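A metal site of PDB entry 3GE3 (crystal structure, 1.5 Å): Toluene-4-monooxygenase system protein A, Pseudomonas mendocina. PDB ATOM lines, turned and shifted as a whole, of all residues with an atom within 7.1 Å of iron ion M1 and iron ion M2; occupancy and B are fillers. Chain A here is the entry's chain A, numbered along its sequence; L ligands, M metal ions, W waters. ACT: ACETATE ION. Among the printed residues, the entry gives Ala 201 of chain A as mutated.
Of the 26 residues printed, 3 come within 4 Å of iron ion M1.
Of the 26 residues printed, 4 come within 4 Å of iron ion M2. The nearest printed residue that does not touch iron ion M2 is Phe 196 (4.9 Å).
Iron ion M2 is bound by OE2 of Glu 231, OE2 of Glu 134, O of the ligand, water W1, OE2 of Glu 197 and NE2 of His 234.
Water W2 bridges the side-chain carboxylate of Glu 104 (2.6 Å) and the side-chain carboxylate of Glu 231 (3.4 Å).
Iron ion M1 is bound by water W1 (2.0 Å), OE2 of Glu 104 (2.0 Å), OE1 of Glu 134 (2.1 Å), OXT of the ligand (2.1 Å), water W2 (2.2 Å) and ND1 of His 137 (2.3 Å).
The backbone carbonyl oxygen of His 137 lies close to the side-chain amide oxygen of Gln 141 (3.0 Å). A ring nitrogen (NE2) of His 137 sits close to the backbone carbonyl oxygen of Asp 133. O of Leu 192 sits at hydrogen-bond distance from N of Glu 197, at 3.1 Å. A ring nitrogen (ND1) of His 234 is in hydrogen-bond range of the side-chain carboxylate (OD2) of Asp 133. The backbone carbonyl oxygen (O) of Ile 227 lies within hydrogen-bond range of a ring nitrogen (NE2) of His 137, at 3.4 Å. A ring nitrogen (ND1) of His 234 lies within hydrogen-bond range of the backbone carbonyl oxygen of Asp 230 (3.4 Å). The side-chain carboxylate of Glu 104 sits close to the side-chain amide oxygen of Gln 141, at 2.9 Å. The side-chain amide nitrogen (NE2) of Gln 228 sits at hydrogen-bond distance from the backbone carbonyl oxygen (O) of Glu 197 (3.3 Å).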
ATOM      1  N   ILE A 100     -11.680 -20.879 -11.767  1.00  0.00           N
ATOM      2  CA  ILE A 100     -13.096 -21.012 -11.394  1.00  0.00           C
ATOM      3  C   ILE A 100     -13.582 -20.067 -10.285  1.00  0.00           C
ATOM      4  O   ILE A 100     -14.672 -19.533 -10.374  1.00  0.00           O
ATOM      5  CB  ILE A 100     -13.364 -22.508 -10.982  1.00  0.00           C
ATOM      6  CG1 ILE A 100     -13.192 -23.412 -12.195  1.00  0.00           C
ATOM      7  CG2 ILE A 100     -14.736 -22.673 -10.307  1.00  0.00           C
ATOM      8  CD1 ILE A 100     -14.225 -23.202 -13.280  1.00  0.00           C
ATOM      9  N   GLY A 103     -14.790 -16.576 -11.160  1.00  0.00           N
ATOM     10  CA  GLY A 103     -15.828 -16.783 -12.176  1.00  0.00           C
ATOM     11  C   GLY A 103     -17.156 -17.212 -11.537  1.00  0.00           C
ATOM     12  O   GLY A 103     -18.224 -16.730 -11.946  1.00  0.00           O
ATOM     13  N   GLU A 104     -17.107 -18.043 -10.507  1.00  0.00           N
ATOM     14  CA  GLU A 104     -18.334 -18.377  -9.753  1.00  0.00           C
ATOM     15  C   GLU A 104     -18.950 -17.115  -9.167  1.00  0.00           C
ATOM     16  O   GLU A 104     -20.176 -16.896  -9.226  1.00  0.00           O
ATOM     17  CB  GLU A 104     -17.961 -19.257  -8.588  1.00  0.00           C
ATOM     18  CG  GLU A 104     -17.432 -20.607  -8.941  1.00  0.00           C
ATOM     19  CD  GLU A 104     -18.492 -21.660  -9.114  1.00  0.00           C
ATOM     20  OE1 GLU A 104     -18.098 -22.835  -9.118  1.00  0.00           O
ATOM     21  OE2 GLU A 104     -19.701 -21.306  -9.241  1.00  0.00           O
ATOM     22  N   TYR A 105     -18.122 -16.255  -8.567  1.00  0.00           N
ATOM     23  CA  TYR A 105     -18.638 -15.022  -8.028  1.00  0.00           C
ATOM     24  C   TYR A 105     -19.231 -14.134  -9.153  1.00  0.00           C
ATOM     25  O   TYR A 105     -20.276 -13.507  -8.945  1.00  0.00           O
ATOM     26  CB  TYR A 105     -17.540 -14.264  -7.255  1.00  0.00           C
ATOM     27  CG  TYR A 105     -18.125 -13.084  -6.571  1.00  0.00           C
ATOM     28  CD1 TYR A 105     -18.924 -13.256  -5.394  1.00  0.00           C
ATOM     29  CD2 TYR A 105     -17.984 -11.793  -7.083  1.00  0.00           C
ATOM     30  CE1 TYR A 105     -19.535 -12.158  -4.763  1.00  0.00           C
ATOM     31  CE2 TYR A 105     -18.555 -10.729  -6.459  1.00  0.00           C
ATOM     32  CZ  TYR A 105     -19.342 -10.871  -5.322  1.00  0.00           C
ATOM     33  OH  TYR A 105     -19.925  -9.751  -4.770  1.00  0.00           O
ATOM     34  N   ALA A 107     -20.750 -15.310 -11.656  1.00  0.00           N
ATOM     35  CA  ALA A 107     -22.019 -15.962 -11.983  1.00  0.00           C
ATOM     36  C   ALA A 107     -23.157 -15.420 -11.116  1.00  0.00           C
ATOM     37  O   ALA A 107     -24.336 -15.493 -11.524  1.00  0.00           O
ATOM     38  CB  ALA A 107     -21.932 -17.466 -11.864  1.00  0.00           C
ATOM     39  N   GLU A 111     -27.114 -14.586 -12.442  1.00  0.00           N
ATOM     40  CA  GLU A 111     -28.357 -14.890 -11.737  1.00  0.00           C
ATOM     41  C   GLU A 111     -29.089 -13.623 -11.351  1.00  0.00           C
ATOM     42  O   GLU A 111     -30.329 -13.585 -11.466  1.00  0.00           O
ATOM     43  CB  GLU A 111     -28.043 -15.768 -10.511  1.00  0.00           C
ATOM     44  CG  GLU A 111     -27.368 -17.142 -10.844  1.00  0.00           C
ATOM     45  CD  GLU A 111     -28.356 -18.177 -11.408  1.00  0.00           C
ATOM     46  OE1 GLU A 111     -29.543 -18.096 -11.139  1.00  0.00           O
ATOM     47  OE2 GLU A 111     -27.922 -19.050 -12.182  1.00  0.00           O
ATOM     48  N   GLY A 130     -30.333 -18.827  -7.032  1.00  0.00           N
ATOM     49  CA  GLY A 130     -29.125 -18.936  -7.877  1.00  0.00           C
ATOM     50  C   GLY A 130     -28.054 -17.948  -7.452  1.00  0.00           C
ATOM     51  O   GLY A 130     -26.858 -18.299  -7.385  1.00  0.00           O
ATOM     52  N   ASP A 133     -26.492 -19.305  -4.361  1.00  0.00           N
ATOM     53  CA  ASP A 133     -25.680 -20.495  -4.654  1.00  0.00           C
ATOM     54  C   ASP A 133     -24.325 -20.051  -5.229  1.00  0.00           C
ATOM     55  O   ASP A 133     -23.296 -20.627  -4.854  1.00  0.00           O
ATOM     56  CB  ASP A 133     -26.310 -21.395  -5.704  1.00  0.00           C
ATOM     57  CG  ASP A 133     -27.598 -22.089  -5.244  1.00  0.00           C
ATOM     58  OD1 ASP A 133     -27.837 -22.285  -4.036  1.00  0.00           O
ATOM     59  OD2 ASP A 133     -28.304 -22.517  -6.148  1.00  0.00           O
ATOM     60  N   GLU A 134     -24.341 -19.096  -6.167  1.00  0.00           N
ATOM     61  CA  GLU A 134     -23.060 -18.743  -6.748  1.00  0.00           C
ATOM     62  C   GLU A 134     -22.192 -17.980  -5.709  1.00  0.00           C
ATOM     63  O   GLU A 134     -20.939 -18.071  -5.766  1.00  0.00           O
ATOM     64  CB  GLU A 134     -23.223 -17.931  -8.023  1.00  0.00           C
ATOM     65  CG  GLU A 134     -24.063 -18.589  -9.089  1.00  0.00           C
ATOM     66  CD  GLU A 134     -23.533 -19.891  -9.643  1.00  0.00           C
ATOM     67  OE1 GLU A 134     -22.498 -20.386  -9.174  1.00  0.00           O
ATOM     68  OE2 GLU A 134     -24.151 -20.390 -10.643  1.00  0.00           O
ATOM     69  N   LEU A 135     -22.820 -17.243  -4.782  1.00  0.00           N
ATOM     70  CA  LEU A 135     -22.061 -16.657  -3.708  1.00  0.00           C
ATOM     71  C   LEU A 135     -21.380 -17.734  -2.898  1.00  0.00           C
ATOM     72  O   LEU A 135     -20.210 -17.639  -2.597  1.00  0.00           O
ATOM     73  CB  LEU A 135     -22.976 -15.820  -2.824  1.00  0.00           C
ATOM     74  CG  LEU A 135     -22.321 -15.147  -1.625  1.00  0.00           C
ATOM     75  CD1 LEU A 135     -21.279 -14.108  -2.130  1.00  0.00           C
ATOM     76  CD2 LEU A 135     -23.338 -14.506  -0.719  1.00  0.00           C
ATOM     77  N   HIS A 137     -20.506 -20.675  -3.941  1.00  0.00           N
ATOM     78  CA  HIS A 137     -19.464 -21.276  -4.738  1.00  0.00           C
ATOM     79  C   HIS A 137     -18.191 -20.432  -4.806  1.00  0.00           C
ATOM     80  O   HIS A 137     -17.079 -20.990  -4.717  1.00  0.00           O
ATOM     81  CB  HIS A 137     -19.934 -21.529  -6.170  1.00  0.00           C
ATOM     82  CG  HIS A 137     -21.104 -22.469  -6.216  1.00  0.00           C
ATOM     83  ND1 HIS A 137     -21.770 -22.789  -7.375  1.00  0.00           N
ATOM     84  CD2 HIS A 137     -21.664 -23.184  -5.229  1.00  0.00           C
ATOM     85  CE1 HIS A 137     -22.770 -23.617  -7.072  1.00  0.00           C
ATOM     86  NE2 HIS A 137     -22.713 -23.885  -5.783  1.00  0.00           N
ATOM     87  N   GLY A 138     -18.386 -19.124  -4.913  1.00  0.00           N
ATOM     88  CA  GLY A 138     -17.222 -18.235  -4.974  1.00  0.00           C
ATOM     89  C   GLY A 138     -16.532 -18.228  -3.608  1.00  0.00           C
ATOM     90  O   GLY A 138     -15.280 -18.267  -3.521  1.00  0.00           O
ATOM     91  N   GLN A 141     -14.641 -21.564  -2.877  1.00  0.00           N
ATOM     92  CA  GLN A 141     -13.460 -21.797  -3.717  1.00  0.00           C
ATOM     93  C   GLN A 141     -12.379 -20.715  -3.566  1.00  0.00           C
ATOM     94  O   GLN A 141     -11.334 -20.833  -4.199  1.00  0.00           O
ATOM     95  CB  GLN A 141     -13.912 -21.994  -5.160  1.00  0.00           C
ATOM     96  CG  GLN A 141     -14.593 -23.384  -5.262  1.00  0.00           C
ATOM     97  CD  GLN A 141     -15.271 -23.613  -6.573  1.00  0.00           C
ATOM     98  OE1 GLN A 141     -16.266 -22.921  -6.922  1.00  0.00           O
ATOM     99  NE2 GLN A 141     -14.812 -24.590  -7.257  1.00  0.00           N
ATOM    100  N   ILE A 180     -22.296 -15.296 -19.393  1.00  0.00           N
ATOM    101  CA  ILE A 180     -22.928 -15.051 -18.073  1.00  0.00           C
ATOM    102  C   ILE A 180     -23.163 -13.612 -17.732  1.00  0.00           C
ATOM    103  O   ILE A 180     -24.272 -13.247 -17.330  1.00  0.00           O
ATOM    104  CB  ILE A 180     -22.078 -15.686 -16.934  1.00  0.00           C
ATOM    105  CG1 ILE A 180     -21.873 -17.149 -17.250  1.00  0.00           C
ATOM    106  CG2 ILE A 180     -22.734 -15.429 -15.571  1.00  0.00           C
ATOM    107  CD1 ILE A 180     -21.099 -17.830 -16.129  1.00  0.00           C
ATOM    108  N   LEU A 192     -26.190 -20.087 -20.115  1.00  0.00           N
ATOM    109  CA  LEU A 192     -25.413 -20.543 -18.967  1.00  0.00           C
ATOM    110  C   LEU A 192     -25.899 -21.906 -18.520  1.00  0.00           C
ATOM    111  O   LEU A 192     -25.093 -22.827 -18.262  1.00  0.00           O
ATOM    112  CB  LEU A 192     -25.520 -19.525 -17.854  1.00  0.00           C
ATOM    113  CG  LEU A 192     -25.154 -19.999 -16.442  1.00  0.00           C
ATOM    114  CD1 LEU A 192     -23.693 -20.413 -16.401  1.00  0.00           C
ATOM    115  CD2 LEU A 192     -25.416 -18.908 -15.434  1.00  0.00           C
ATOM    116  N   PHE A 196     -22.530 -24.547 -19.540  1.00  0.00           N
ATOM    117  CA  PHE A 196     -21.748 -24.853 -18.343  1.00  0.00           C
ATOM    118  C   PHE A 196     -22.572 -25.700 -17.359  1.00  0.00           C
ATOM    119  O   PHE A 196     -22.169 -26.813 -16.991  1.00  0.00           O
ATOM    120  CB  PHE A 196     -21.258 -23.571 -17.680  1.00  0.00           C
ATOM    121  CG  PHE A 196     -20.481 -23.816 -16.438  1.00  0.00           C
ATOM    122  CD1 PHE A 196     -19.216 -24.382 -16.476  1.00  0.00           C
ATOM    123  CD2 PHE A 196     -21.062 -23.628 -15.231  1.00  0.00           C
ATOM    124  CE1 PHE A 196     -18.524 -24.666 -15.281  1.00  0.00           C
ATOM    125  CE2 PHE A 196     -20.376 -23.885 -14.033  1.00  0.00           C
ATOM    126  CZ  PHE A 196     -19.129 -24.382 -14.065  1.00  0.00           C
ATOM    127  N   GLU A 197     -23.744 -25.222 -16.918  1.00  0.00           N
ATOM    128  CA  GLU A 197     -24.307 -25.787 -15.678  1.00  0.00           C
ATOM    129  C   GLU A 197     -24.762 -27.229 -15.799  1.00  0.00           C
ATOM    130  O   GLU A 197     -24.465 -28.020 -14.923  1.00  0.00           O
ATOM    131  CB  GLU A 197     -25.466 -24.894 -15.177  1.00  0.00           C
ATOM    132  CG  GLU A 197     -24.918 -23.498 -14.877  1.00  0.00           C
ATOM    133  CD  GLU A 197     -25.889 -22.655 -14.121  1.00  0.00           C
ATOM    134  OE1 GLU A 197     -27.095 -22.736 -14.438  1.00  0.00           O
ATOM    135  OE2 GLU A 197     -25.481 -21.869 -13.228  1.00  0.00           O
ATOM    136  N   ALA A 201     -19.846 -28.162 -16.553  1.00  0.00           N
ATOM    137  CA  ALA A 201     -19.634 -28.201 -15.111  1.00  0.00           C
ATOM    138  C   ALA A 201     -19.533 -29.626 -14.634  1.00  0.00           C
ATOM    139  O   ALA A 201     -18.791 -29.924 -13.696  1.00  0.00           O
ATOM    140  CB  ALA A 201     -20.759 -27.508 -14.343  1.00  0.00           C
ATOM    141  N   PHE A 205     -16.454 -30.662 -12.259  1.00  0.00           N
ATOM    142  CA  PHE A 205     -16.898 -30.803 -10.854  1.00  0.00           C
ATOM    143  C   PHE A 205     -17.322 -32.237 -10.424  1.00  0.00           C
ATOM    144  O   PHE A 205     -17.512 -32.519  -9.182  1.00  0.00           O
ATOM    145  CB  PHE A 205     -18.069 -29.854 -10.593  1.00  0.00           C
ATOM    146  CG  PHE A 205     -17.681 -28.408 -10.540  1.00  0.00           C
ATOM    147  CD1 PHE A 205     -17.467 -27.730 -11.725  1.00  0.00           C
ATOM    148  CD2 PHE A 205     -17.440 -27.765  -9.340  1.00  0.00           C
ATOM    149  CE1 PHE A 205     -17.116 -26.373 -11.685  1.00  0.00           C
ATOM    150  CE2 PHE A 205     -17.073 -26.426  -9.296  1.00  0.00           C
ATOM    151  CZ  PHE A 205     -16.916 -25.750 -10.466  1.00  0.00           C
ATOM    152  N   ILE A 227     -20.801 -28.618  -4.538  1.00  0.00           N
ATOM    153  CA  ILE A 227     -21.102 -27.455  -5.333  1.00  0.00           C
ATOM    154  C   ILE A 227     -22.075 -27.869  -6.475  1.00  0.00           C
ATOM    155  O   ILE A 227     -23.047 -27.161  -6.769  1.00  0.00           O
ATOM    156  CB  ILE A 227     -19.774 -26.841  -5.843  1.00  0.00           C
ATOM    157  CG1 ILE A 227     -19.109 -26.120  -4.662  1.00  0.00           C
ATOM    158  CG2 ILE A 227     -20.035 -25.956  -7.073  1.00  0.00           C
ATOM    159  CD1 ILE A 227     -17.686 -25.553  -5.039  1.00  0.00           C
ATOM    160  N   GLN A 228     -21.819 -29.018  -7.112  1.00  0.00           N
ATOM    161  CA  GLN A 228     -22.641 -29.438  -8.249  1.00  0.00           C
ATOM    162  C   GLN A 228     -24.080 -29.756  -7.837  1.00  0.00           C
ATOM    163  O   GLN A 228     -24.966 -29.621  -8.668  1.00  0.00           O
ATOM    164  CB  GLN A 228     -21.983 -30.593  -9.002  1.00  0.00           C
ATOM    165  CG  GLN A 228     -22.475 -30.779 -10.436  1.00  0.00           C
ATOM    166  CD  GLN A 228     -22.296 -29.585 -11.364  1.00  0.00           C
ATOM    167  OE1 GLN A 228     -21.644 -28.604 -11.036  1.00  0.00           O
ATOM    168  NE2 GLN A 228     -22.923 -29.675 -12.536  1.00  0.00           N
ATOM    169  N   ASP A 230     -25.889 -27.830  -6.040  1.00  0.00           N
ATOM    170  CA  ASP A 230     -26.636 -26.592  -6.168  1.00  0.00           C
ATOM    171  C   ASP A 230     -26.872 -26.302  -7.626  1.00  0.00           C
ATOM    172  O   ASP A 230     -27.958 -25.871  -8.003  1.00  0.00           O
ATOM    173  CB  ASP A 230     -25.778 -25.432  -5.644  1.00  0.00           C
ATOM    174  CG  ASP A 230     -25.414 -25.536  -4.196  1.00  0.00           C
ATOM    175  OD1 ASP A 230     -26.213 -25.964  -3.324  1.00  0.00           O
ATOM    176  OD2 ASP A 230     -24.310 -25.092  -3.884  1.00  0.00           O
ATOM    177  N   GLU A 231     -25.820 -26.510  -8.449  1.00  0.00           N
ATOM    178  CA  GLU A 231     -25.939 -26.331  -9.884  1.00  0.00           C
ATOM    179  C   GLU A 231     -27.115 -27.112 -10.463  1.00  0.00           C
ATOM    180  O   GLU A 231     -27.872 -26.635 -11.322  1.00  0.00           O
ATOM    181  CB  GLU A 231     -24.625 -26.790 -10.538  1.00  0.00           C
ATOM    182  CG  GLU A 231     -24.503 -26.448 -11.981  1.00  0.00           C
ATOM    183  CD  GLU A 231     -23.764 -25.141 -12.160  1.00  0.00           C
ATOM    184  OE1 GLU A 231     -22.500 -25.202 -12.211  1.00  0.00           O
ATOM    185  OE2 GLU A 231     -24.387 -24.046 -12.155  1.00  0.00           O
ATOM    186  N   SER A 232     -27.240 -28.363 -10.027  1.00  0.00           N
ATOM    187  CA  SER A 232     -28.242 -29.254 -10.599  1.00  0.00           C
ATOM    188  C   SER A 232     -29.640 -28.740 -10.283  1.00  0.00           C
ATOM    189  O   SER A 232     -30.584 -29.024 -11.020  1.00  0.00           O
ATOM    190  CB  SER A 232     -27.957 -30.675 -10.144  1.00  0.00           C
ATOM    191  OG  SER A 232     -26.779 -31.026 -10.912  1.00  0.00           O
ATOM    192  N   HIS A 234     -30.258 -25.027  -9.616  1.00  0.00           N
ATOM    193  CA  HIS A 234     -30.525 -23.738 -10.265  1.00  0.00           C
ATOM    194  C   HIS A 234     -30.420 -23.810 -11.778  1.00  0.00           C
ATOM    195  O   HIS A 234     -30.991 -22.943 -12.470  1.00  0.00           O
ATOM    196  CB  HIS A 234     -29.657 -22.574  -9.669  1.00  0.00           C
ATOM    197  CG  HIS A 234     -28.157 -22.668  -9.822  1.00  0.00           C
ATOM    198  ND1 HIS A 234     -27.329 -22.609  -8.724  1.00  0.00           N
ATOM    199  CD2 HIS A 234     -27.344 -22.677 -10.912  1.00  0.00           C
ATOM    200  CE1 HIS A 234     -26.070 -22.587  -9.118  1.00  0.00           C
ATOM    201  NE2 HIS A 234     -26.033 -22.621 -10.445  1.00  0.00           N
ATOM    202  N   ALA A 235     -29.755 -24.830 -12.316  1.00  0.00           N
ATOM    203  CA  ALA A 235     -29.660 -24.959 -13.801  1.00  0.00           C
ATOM    204  C   ALA A 235     -31.027 -25.261 -14.380  1.00  0.00           C
ATOM    205  O   ALA A 235     -31.210 -25.096 -15.605  1.00  0.00           O
ATOM    206  CB  ALA A 235     -28.697 -26.080 -14.191  1.00  0.00           C
HETATM  207  C   ACT L   1     -21.527 -21.223 -12.627  1.00  0.00           C
HETATM  208  O   ACT L   1     -22.734 -21.564 -12.837  1.00  0.00           O
HETATM  209  OXT ACT L   1     -21.059 -21.463 -11.481  1.00  0.00           O
HETATM  210  CH3 ACT L   1     -20.753 -20.512 -13.695  1.00  0.00           C
HETATM  211 FE    FE M   1     -21.484 -22.184  -9.537  1.00  0.00          FE
HETATM  212 FE    FE M   2     -24.212 -22.228 -11.565  1.00  0.00          FE
HETATM  213  O   HOH W   1     -23.093 -23.175 -10.047  1.00  0.00           O
HETATM  214  O   HOH W   2     -20.304 -24.002  -9.958  1.00  0.00           O
